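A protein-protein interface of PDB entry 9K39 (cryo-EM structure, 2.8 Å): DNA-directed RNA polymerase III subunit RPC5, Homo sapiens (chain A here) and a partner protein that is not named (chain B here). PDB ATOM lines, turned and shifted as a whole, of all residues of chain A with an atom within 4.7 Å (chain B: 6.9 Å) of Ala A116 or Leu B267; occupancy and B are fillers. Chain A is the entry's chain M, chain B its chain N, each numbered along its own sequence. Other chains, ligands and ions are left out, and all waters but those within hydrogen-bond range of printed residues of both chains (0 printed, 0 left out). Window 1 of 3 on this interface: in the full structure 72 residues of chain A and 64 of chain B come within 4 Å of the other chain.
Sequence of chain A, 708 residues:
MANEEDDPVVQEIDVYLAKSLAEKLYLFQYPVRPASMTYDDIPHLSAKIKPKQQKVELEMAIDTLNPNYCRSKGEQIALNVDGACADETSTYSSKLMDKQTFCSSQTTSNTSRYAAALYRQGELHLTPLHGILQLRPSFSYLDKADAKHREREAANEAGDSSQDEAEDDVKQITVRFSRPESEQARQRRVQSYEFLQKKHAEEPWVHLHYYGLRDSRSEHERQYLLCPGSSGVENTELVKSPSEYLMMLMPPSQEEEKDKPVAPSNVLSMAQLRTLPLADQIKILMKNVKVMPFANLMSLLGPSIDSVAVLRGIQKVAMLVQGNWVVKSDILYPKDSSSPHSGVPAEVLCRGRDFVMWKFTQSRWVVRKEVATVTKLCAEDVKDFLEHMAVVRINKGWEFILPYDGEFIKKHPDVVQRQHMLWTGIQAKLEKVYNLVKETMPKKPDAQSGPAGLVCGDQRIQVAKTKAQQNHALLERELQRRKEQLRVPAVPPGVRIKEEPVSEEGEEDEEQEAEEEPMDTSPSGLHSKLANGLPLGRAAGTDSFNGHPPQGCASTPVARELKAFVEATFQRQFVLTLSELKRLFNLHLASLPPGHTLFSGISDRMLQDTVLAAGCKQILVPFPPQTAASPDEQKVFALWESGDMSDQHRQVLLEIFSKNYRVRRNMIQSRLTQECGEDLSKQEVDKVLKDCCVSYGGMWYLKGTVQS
O of Ala A115 lies within hydrogen-bond range of N of Leu B269 (3.4 Å).
The backbone carbonyl oxygen (O) of Ala A117 is in hydrogen-bond range of the backbone NH (N) of Leu B267 (2.5 Å).
O of Leu B360 lies within hydrogen-bond range of N of Leu B376 (2.9 Å).
The backbone carbonyl oxygen of His B381 sits at hydrogen-bond distance from the backbone NH of Phe B268 (3.5 Å).
N of His A125 lies within hydrogen-bond range of O of Leu A118 (2.9 Å).
N of Ala A116 lies within hydrogen-bond range of O of Thr A127.
N of Leu B383 is in hydrogen-bond range of O of Phe B268 (3.0 Å).
Leu A25 touches Leu B360.
CD1 of Leu A25 touches CD1 of Leu B376, at 3.7 Å.
Tyr A114 touches Phe B268.
Phe B268 touches Ala A115 (CD1 to O, 3.5 Å).
Ala A115 touches Leu B318 (CB to CD1, 3.7 Å).
Ala A117 touches Glu B265 (O to O, 3.9 Å).
Ala A117 touches Leu B266 (O to C, 3.4 Å).
Leu A118 touches Leu B266 (CB to CD1, 3.7 Å).
Leu A124 touches Leu B269 (CD2 to CD2, 3.8 Å).
Leu A129 touches Phe B268.
Printed residues of chain A within 4 Å of Leu B267: Ala A116 (3.6 Å) and Ala A117 (2.5 Å).
Of the printed residues of chain A, Leu B266 touches Ala A117 (3.4 Å) and Leu A118 (3.7 Å).
Of the printed residues of chain A, Leu B318 touches Ala A115 (3.7 Å).
His B381 touches none of the printed residues of chain A.
Thr A127 touches none of the printed residues of chain B.
The nearest residue of chain B that does not touch Ala A116 is Phe B268 (4.7 Å).
The nearest printed residue of chain A that does not touch Leu B267 is Ala A115 (4.5 Å).
Of the 11 printed residues of chain A, 9 touch a printed residue of chain B.
Among the printed residues, 17 pairs touch across the chains.
Among the printed residues, no Asp or Glu carboxylate lies within 4 Å of a Lys or Arg side-chain nitrogen of the other chain.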
ATOM      1  N   LEU A  25       7.014  25.523  14.694  1.00  0.00           N
ATOM      2  CA  LEU A  25       8.003  24.449  14.687  1.00  0.00           C
ATOM      3  C   LEU A  25       7.317  23.123  15.000  1.00  0.00           C
ATOM      4  O   LEU A  25       6.721  22.966  16.072  1.00  0.00           O
ATOM      5  CB  LEU A  25       9.116  24.729  15.696  1.00  0.00           C
ATOM      6  CG  LEU A  25      10.317  23.787  15.669  1.00  0.00           C
ATOM      7  CD1 LEU A  25      10.979  23.818  14.304  1.00  0.00           C
ATOM      8  CD2 LEU A  25      11.313  24.156  16.756  1.00  0.00           C
ATOM      9  N   TYR A 114       9.432  20.001  25.539  1.00  0.00           N
ATOM     10  CA  TYR A 114      10.312  19.594  24.455  1.00  0.00           C
ATOM     11  C   TYR A 114      10.784  20.817  23.684  1.00  0.00           C
ATOM     12  O   TYR A 114      10.021  21.767  23.479  1.00  0.00           O
ATOM     13  CB  TYR A 114       9.602  18.619  23.513  1.00  0.00           C
ATOM     14  CG  TYR A 114       9.041  17.399  24.208  1.00  0.00           C
ATOM     15  CD1 TYR A 114       9.844  16.300  24.482  1.00  0.00           C
ATOM     16  CD2 TYR A 114       7.706  17.345  24.589  1.00  0.00           C
ATOM     17  CE1 TYR A 114       9.336  15.185  25.117  1.00  0.00           C
ATOM     18  CE2 TYR A 114       7.188  16.233  25.224  1.00  0.00           C
ATOM     19  CZ  TYR A 114       8.007  15.156  25.487  1.00  0.00           C
ATOM     20  OH  TYR A 114       7.495  14.046  26.119  1.00  0.00           O
ATOM     21  N   ALA A 115      12.045  20.792  23.256  1.00  0.00           N
ATOM     22  CA  ALA A 115      12.644  21.919  22.557  1.00  0.00           C
ATOM     23  C   ALA A 115      13.676  21.421  21.557  1.00  0.00           C
ATOM     24  O   ALA A 115      14.347  20.412  21.788  1.00  0.00           O
ATOM     25  CB  ALA A 115      13.300  22.900  23.536  1.00  0.00           C
ATOM     26  N   ALA A 116      13.794  22.139  20.441  1.00  0.00           N
ATOM     27  CA  ALA A 116      14.797  21.852  19.427  1.00  0.00           C
ATOM     28  C   ALA A 116      16.038  22.689  19.695  1.00  0.00           C
ATOM     29  O   ALA A 116      15.936  23.889  19.976  1.00  0.00           O
ATOM     30  CB  ALA A 116      14.252  22.139  18.028  1.00  0.00           C
ATOM     31  N   ALA A 117      17.207  22.056  19.615  1.00  0.00           N
ATOM     32  CA  ALA A 117      18.478  22.685  19.956  1.00  0.00           C
ATOM     33  C   ALA A 117      19.355  22.747  18.711  1.00  0.00           C
ATOM     34  O   ALA A 117      19.773  21.708  18.188  1.00  0.00           O
ATOM     35  CB  ALA A 117      19.174  21.922  21.081  1.00  0.00           C
ATOM     36  N   LEU A 118      19.628  23.962  18.241  1.00  0.00           N
ATOM     37  CA  LEU A 118      20.559  24.178  17.144  1.00  0.00           C
ATOM     38  C   LEU A 118      21.911  24.595  17.716  1.00  0.00           C
ATOM     39  O   LEU A 118      22.003  25.590  18.442  1.00  0.00           O
ATOM     40  CB  LEU A 118      20.026  25.243  16.181  1.00  0.00           C
ATOM     41  CG  LEU A 118      20.746  25.417  14.840  1.00  0.00           C
ATOM     42  CD1 LEU A 118      19.756  25.778  13.746  1.00  0.00           C
ATOM     43  CD2 LEU A 118      21.829  26.479  14.934  1.00  0.00           C
ATOM     44  N   LEU A 124      24.279  27.394  21.852  1.00  0.00           N
ATOM     45  CA  LEU A 124      23.193  26.447  21.636  1.00  0.00           C
ATOM     46  C   LEU A 124      21.876  27.201  21.734  1.00  0.00           C
ATOM     47  O   LEU A 124      21.546  27.737  22.797  1.00  0.00           O
ATOM     48  CB  LEU A 124      23.241  25.306  22.656  1.00  0.00           C
ATOM     49  CG  LEU A 124      22.231  24.175  22.456  1.00  0.00           C
ATOM     50  CD1 LEU A 124      22.486  23.463  21.137  1.00  0.00           C
ATOM     51  CD2 LEU A 124      22.282  23.196  23.617  1.00  0.00           C
ATOM     52  N   HIS A 125      21.131  27.249  20.633  1.00  0.00           N
ATOM     53  CA  HIS A 125      19.867  27.971  20.569  1.00  0.00           C
ATOM     54  C   HIS A 125      18.710  26.997  20.757  1.00  0.00           C
ATOM     55  O   HIS A 125      18.627  25.984  20.056  1.00  0.00           O
ATOM     56  CB  HIS A 125      19.724  28.704  19.235  1.00  0.00           C
ATOM     57  CG  HIS A 125      20.781  29.738  18.994  1.00  0.00           C
ATOM     58  ND1 HIS A 125      20.505  31.088  18.952  1.00  0.00           N
ATOM     59  CD2 HIS A 125      22.114  29.619  18.785  1.00  0.00           C
ATOM     60  CE1 HIS A 125      21.621  31.757  18.726  1.00  0.00           C
ATOM     61  NE2 HIS A 125      22.612  30.890  18.621  1.00  0.00           N
ATOM     62  N   LEU A 126      17.823  27.311  21.697  1.00  0.00           N
ATOM     63  CA  LEU A 126      16.663  26.481  21.988  1.00  0.00           C
ATOM     64  C   LEU A 126      15.407  27.120  21.411  1.00  0.00           C
ATOM     65  O   LEU A 126      15.234  28.340  21.474  1.00  0.00           O
ATOM     66  CB  LEU A 126      16.501  26.281  23.496  1.00  0.00           C
ATOM     67  CG  LEU A 126      17.719  25.748  24.248  1.00  0.00           C
ATOM     68  CD1 LEU A 126      17.381  25.502  25.712  1.00  0.00           C
ATOM     69  CD2 LEU A 126      18.245  24.481  23.594  1.00  0.00           C
ATOM     70  N   THR A 127      14.529  26.285  20.851  1.00  0.00           N
ATOM     71  CA  THR A 127      13.276  26.757  20.279  1.00  0.00           C
ATOM     72  C   THR A 127      12.157  25.814  20.705  1.00  0.00           C
ATOM     73  O   THR A 127      12.270  24.591  20.503  1.00  0.00           O
ATOM     74  CB  THR A 127      13.347  26.847  18.752  1.00  0.00           C
ATOM     75  OG1 THR A 127      14.469  27.654  18.372  1.00  0.00           O
ATOM     76  CG2 THR A 127      12.074  27.468  18.197  1.00  0.00           C
ATOM     77  N   LEU A 129       8.679  23.650  20.805  1.00  0.00           N
ATOM     78  CA  LEU A 129       7.957  22.884  19.797  1.00  0.00           C
ATOM     79  C   LEU A 129       6.458  23.053  19.997  1.00  0.00           C
ATOM     80  O   LEU A 129       5.945  22.845  21.102  1.00  0.00           O
ATOM     81  CB  LEU A 129       8.331  21.400  19.860  1.00  0.00           C
ATOM     82  CG  LEU A 129       9.492  20.924  18.984  1.00  0.00           C
ATOM     83  CD1 LEU A 129      10.779  21.635  19.349  1.00  0.00           C
ATOM     84  CD2 LEU A 129       9.668  19.417  19.100  1.00  0.00           C
ATOM     85  N   GLU B 253      30.699  13.750  22.991  1.00  0.00           N
ATOM     86  CA  GLU B 253      29.853  14.162  21.877  1.00  0.00           C
ATOM     87  C   GLU B 253      30.101  15.622  21.514  1.00  0.00           C
ATOM     88  O   GLU B 253      30.406  15.948  20.362  1.00  0.00           O
ATOM     89  CB  GLU B 253      28.380  13.932  22.231  1.00  0.00           C
ATOM     90  CG  GLU B 253      27.400  14.350  21.144  1.00  0.00           C
ATOM     91  CD  GLU B 253      27.426  13.430  19.939  1.00  0.00           C
ATOM     92  OE1 GLU B 253      27.960  12.308  20.051  1.00  0.00           O
ATOM     93  OE2 GLU B 253      26.910  13.831  18.871  1.00  0.00           O
ATOM     94  N   LEU B 254      29.981  16.519  22.497  1.00  0.00           N
ATOM     95  CA  LEU B 254      30.221  17.935  22.235  1.00  0.00           C
ATOM     96  C   LEU B 254      31.674  18.191  21.850  1.00  0.00           C
ATOM     97  O   LEU B 254      31.956  19.063  21.016  1.00  0.00           O
ATOM     98  CB  LEU B 254      29.831  18.768  23.457  1.00  0.00           C
ATOM     99  CG  LEU B 254      28.361  18.701  23.875  1.00  0.00           C
ATOM    100  CD1 LEU B 254      28.100  19.595  25.076  1.00  0.00           C
ATOM    101  CD2 LEU B 254      27.456  19.080  22.714  1.00  0.00           C
ATOM    102  N   GLU B 257      31.984  17.316  18.352  1.00  0.00           N
ATOM    103  CA  GLU B 257      31.170  18.228  17.557  1.00  0.00           C
ATOM    104  C   GLU B 257      31.837  19.588  17.385  1.00  0.00           C
ATOM    105  O   GLU B 257      31.574  20.279  16.393  1.00  0.00           O
ATOM    106  CB  GLU B 257      29.790  18.398  18.194  1.00  0.00           C
ATOM    107  CG  GLU B 257      28.834  17.247  17.931  1.00  0.00           C
ATOM    108  CD  GLU B 257      27.469  17.469  18.556  1.00  0.00           C
ATOM    109  OE1 GLU B 257      27.311  18.457  19.302  1.00  0.00           O
ATOM    110  OE2 GLU B 257      26.559  16.656  18.301  1.00  0.00           O
ATOM    111  N   GLU B 265      25.102  21.217  14.155  1.00  0.00           N
ATOM    112  CA  GLU B 265      24.315  20.020  14.407  1.00  0.00           C
ATOM    113  C   GLU B 265      23.018  20.403  15.104  1.00  0.00           C
ATOM    114  O   GLU B 265      22.991  21.295  15.956  1.00  0.00           O
ATOM    115  CB  GLU B 265      25.096  19.008  15.260  1.00  0.00           C
ATOM    116  CG  GLU B 265      24.353  17.710  15.544  1.00  0.00           C
ATOM    117  CD  GLU B 265      24.131  16.873  14.298  1.00  0.00           C
ATOM    118  OE1 GLU B 265      24.893  17.038  13.322  1.00  0.00           O
ATOM    119  OE2 GLU B 265      23.192  16.050  14.295  1.00  0.00           O
ATOM    120  N   LEU B 266      21.941  19.716  14.731  1.00  0.00           N
ATOM    121  CA  LEU B 266      20.623  19.926  15.320  1.00  0.00           C
ATOM    122  C   LEU B 266      20.397  18.884  16.406  1.00  0.00           C
ATOM    123  O   LEU B 266      20.470  17.680  16.142  1.00  0.00           O
ATOM    124  CB  LEU B 266      19.525  19.844  14.259  1.00  0.00           C
ATOM    125  CG  LEU B 266      19.165  21.124  13.498  1.00  0.00           C
ATOM    126  CD1 LEU B 266      18.723  22.214  14.462  1.00  0.00           C
ATOM    127  CD2 LEU B 266      20.319  21.602  12.630  1.00  0.00           C
ATOM    128  N   LEU B 267      20.122  19.348  17.622  1.00  0.00           N
ATOM    129  CA  LEU B 267      19.884  18.478  18.762  1.00  0.00           C
ATOM    130  C   LEU B 267      18.449  18.627  19.249  1.00  0.00           C
ATOM    131  O   LEU B 267      17.776  19.626  18.984  1.00  0.00           O
ATOM    132  CB  LEU B 267      20.859  18.788  19.903  1.00  0.00           C
ATOM    133  CG  LEU B 267      22.349  18.642  19.587  1.00  0.00           C
ATOM    134  CD1 LEU B 267      23.194  19.003  20.798  1.00  0.00           C
ATOM    135  CD2 LEU B 267      22.659  17.230  19.114  1.00  0.00           C
ATOM    136  N   PHE B 268      17.984  17.608  19.970  1.00  0.00           N
ATOM    137  CA  PHE B 268      16.642  17.589  20.550  1.00  0.00           C
ATOM    138  C   PHE B 268      16.780  17.222  22.025  1.00  0.00           C
ATOM    139  O   PHE B 268      16.908  16.043  22.368  1.00  0.00           O
ATOM    140  CB  PHE B 268      15.736  16.607  19.811  1.00  0.00           C
ATOM    141  CG  PHE B 268      14.366  16.476  20.413  1.00  0.00           C
ATOM    142  CD1 PHE B 268      13.397  17.440  20.187  1.00  0.00           C
ATOM    143  CD2 PHE B 268      14.043  15.382  21.198  1.00  0.00           C
ATOM    144  CE1 PHE B 268      12.135  17.318  20.737  1.00  0.00           C
ATOM    145  CE2 PHE B 268      12.784  15.254  21.752  1.00  0.00           C
ATOM    146  CZ  PHE B 268      11.828  16.224  21.521  1.00  0.00           C
ATOM    147  N   LEU B 269      16.754  18.228  22.892  1.00  0.00           N
ATOM    148  CA  LEU B 269      16.897  18.031  24.327  1.00  0.00           C
ATOM    149  C   LEU B 269      15.542  18.157  25.011  1.00  0.00           C
ATOM    150  O   LEU B 269      14.691  18.946  24.589  1.00  0.00           O
ATOM    151  CB  LEU B 269      17.894  19.031  24.926  1.00  0.00           C
ATOM    152  CG  LEU B 269      17.894  20.490  24.457  1.00  0.00           C
ATOM    153  CD1 LEU B 269      16.796  21.308  25.122  1.00  0.00           C
ATOM    154  CD2 LEU B 269      19.257  21.112  24.717  1.00  0.00           C
ATOM    155  N   LEU B 318       9.626  27.416  28.301  1.00  0.00           N
ATOM    156  CA  LEU B 318      10.337  28.314  27.398  1.00  0.00           C
ATOM    157  C   LEU B 318       9.408  29.318  26.725  1.00  0.00           C
ATOM    158  O   LEU B 318       9.882  30.353  26.247  1.00  0.00           O
ATOM    159  CB  LEU B 318      11.082  27.510  26.331  1.00  0.00           C
ATOM    160  CG  LEU B 318      12.159  26.538  26.821  1.00  0.00           C
ATOM    161  CD1 LEU B 318      12.849  25.878  25.641  1.00  0.00           C
ATOM    162  CD2 LEU B 318      13.167  27.254  27.703  1.00  0.00           C
ATOM    163  N   LEU B 360      13.473  17.693  11.548  1.00  0.00           N
ATOM    164  CA  LEU B 360      12.996  18.916  12.175  1.00  0.00           C
ATOM    165  C   LEU B 360      12.633  19.915  11.085  1.00  0.00           C
ATOM    166  O   LEU B 360      13.505  20.375  10.338  1.00  0.00           O
ATOM    167  CB  LEU B 360      14.062  19.491  13.105  1.00  0.00           C
ATOM    168  CG  LEU B 360      13.710  20.788  13.837  1.00  0.00           C
ATOM    169  CD1 LEU B 360      12.615  20.545  14.865  1.00  0.00           C
ATOM    170  CD2 LEU B 360      14.946  21.387  14.489  1.00  0.00           C
ATOM    171  N   LEU B 376      13.996  22.248   8.233  1.00  0.00           N
ATOM    172  CA  LEU B 376      15.149  22.911   8.829  1.00  0.00           C
ATOM    173  C   LEU B 376      16.367  21.997   8.856  1.00  0.00           C
ATOM    174  O   LEU B 376      17.488  22.439   8.581  1.00  0.00           O
ATOM    175  CB  LEU B 376      14.804  23.397  10.236  1.00  0.00           C
ATOM    176  CG  LEU B 376      13.676  24.425  10.318  1.00  0.00           C
ATOM    177  CD1 LEU B 376      13.404  24.816  11.760  1.00  0.00           C
ATOM    178  CD2 LEU B 376      14.007  25.652   9.482  1.00  0.00           C
ATOM    179  N   HIS B 378      17.856  17.626  10.074  1.00  0.00           N
ATOM    180  CA  HIS B 378      17.638  16.276  10.566  1.00  0.00           C
ATOM    181  C   HIS B 378      18.063  16.176  12.025  1.00  0.00           C
ATOM    182  O   HIS B 378      19.032  16.817  12.447  1.00  0.00           O
ATOM    183  CB  HIS B 378      18.409  15.256   9.724  1.00  0.00           C
ATOM    184  CG  HIS B 378      17.998  15.228   8.285  1.00  0.00           C
ATOM    185  ND1 HIS B 378      16.934  14.483   7.828  1.00  0.00           N
ATOM    186  CD2 HIS B 378      18.513  15.857   7.200  1.00  0.00           C
ATOM    187  CE1 HIS B 378      16.808  14.653   6.523  1.00  0.00           C
ATOM    188  NE2 HIS B 378      17.753  15.483   6.119  1.00  0.00           N
ATOM    189  N   VAL B 379      17.334  15.368  12.792  1.00  0.00           N
ATOM    190  CA  VAL B 379      17.616  15.146  14.205  1.00  0.00           C
ATOM    191  C   VAL B 379      18.240  13.765  14.359  1.00  0.00           C
ATOM    192  O   VAL B 379      17.687  12.768  13.884  1.00  0.00           O
ATOM    193  CB  VAL B 379      16.342  15.272  15.055  1.00  0.00           C
ATOM    194  CG1 VAL B 379      16.659  15.046  16.525  1.00  0.00           C
ATOM    195  CG2 VAL B 379      15.700  16.635  14.848  1.00  0.00           C
ATOM    196  N   LYS B 380      19.395  13.709  15.023  1.00  0.00           N
ATOM    197  CA  LYS B 380      20.133  12.464  15.206  1.00  0.00           C
ATOM    198  C   LYS B 380      20.283  12.074  16.667  1.00  0.00           C
ATOM    199  O   LYS B 380      20.037  10.915  17.023  1.00  0.00           O
ATOM    200  CB  LYS B 380      21.519  12.580  14.556  1.00  0.00           C
ATOM    201  CG  LYS B 380      22.358  11.315  14.650  1.00  0.00           C
ATOM    202  CD  LYS B 380      21.716  10.167  13.889  1.00  0.00           C
ATOM    203  CE  LYS B 380      21.626  10.476  12.402  1.00  0.00           C
ATOM    204  NZ  LYS B 380      22.967  10.721  11.803  1.00  0.00           N
ATOM    205  N   HIS B 381      20.672  13.009  17.529  1.00  0.00           N
ATOM    206  CA  HIS B 381      20.907  12.729  18.937  1.00  0.00           C
ATOM    207  C   HIS B 381      19.832  13.392  19.787  1.00  0.00           C
ATOM    208  O   HIS B 381      19.257  14.417  19.407  1.00  0.00           O
ATOM    209  CB  HIS B 381      22.292  13.216  19.380  1.00  0.00           C
ATOM    210  CG  HIS B 381      23.418  12.661  18.564  1.00  0.00           C
ATOM    211  ND1 HIS B 381      23.763  13.168  17.329  1.00  0.00           N
ATOM    212  CD2 HIS B 381      24.273  11.639  18.803  1.00  0.00           C
ATOM    213  CE1 HIS B 381      24.785  12.485  16.843  1.00  0.00           C
ATOM    214  NE2 HIS B 381      25.113  11.551  17.718  1.00  0.00           N
ATOM    215  N   LYS B 382      19.565  12.794  20.946  1.00  0.00           N
ATOM    216  CA  LYS B 382      18.580  13.298  21.893  1.00  0.00           C
ATOM    217  C   LYS B 382      19.230  13.460  23.258  1.00  0.00           C
ATOM    218  O   LYS B 382      19.909  12.546  23.738  1.00  0.00           O
ATOM    219  CB  LYS B 382      17.374  12.363  21.985  1.00  0.00           C
ATOM    220  CG  LYS B 382      16.301  12.826  22.959  1.00  0.00           C
ATOM    221  CD  LYS B 382      15.142  11.846  23.015  1.00  0.00           C
ATOM    222  CE  LYS B 382      14.089  12.293  24.018  1.00  0.00           C
ATOM    223  NZ  LYS B 382      12.961  11.328  24.112  1.00  0.00           N
ATOM    224  N   LEU B 383      19.023  14.618  23.876  1.00  0.00           N
ATOM    225  CA  LEU B 383      19.551  14.919  25.198  1.00  0.00           C
ATOM    226  C   LEU B 383      18.417  14.976  26.214  1.00  0.00           C
ATOM    227  O   LEU B 383      17.260  15.226  25.864  1.00  0.00           O
ATOM    228  CB  LEU B 383      20.317  16.248  25.197  1.00  0.00           C
ATOM    229  CG  LEU B 383      21.486  16.370  24.220  1.00  0.00           C
ATOM    230  CD1 LEU B 383      22.122  17.748  24.313  1.00  0.00           C
ATOM    231  CD2 LEU B 383      22.517  15.282  24.473  1.00  0.00           C
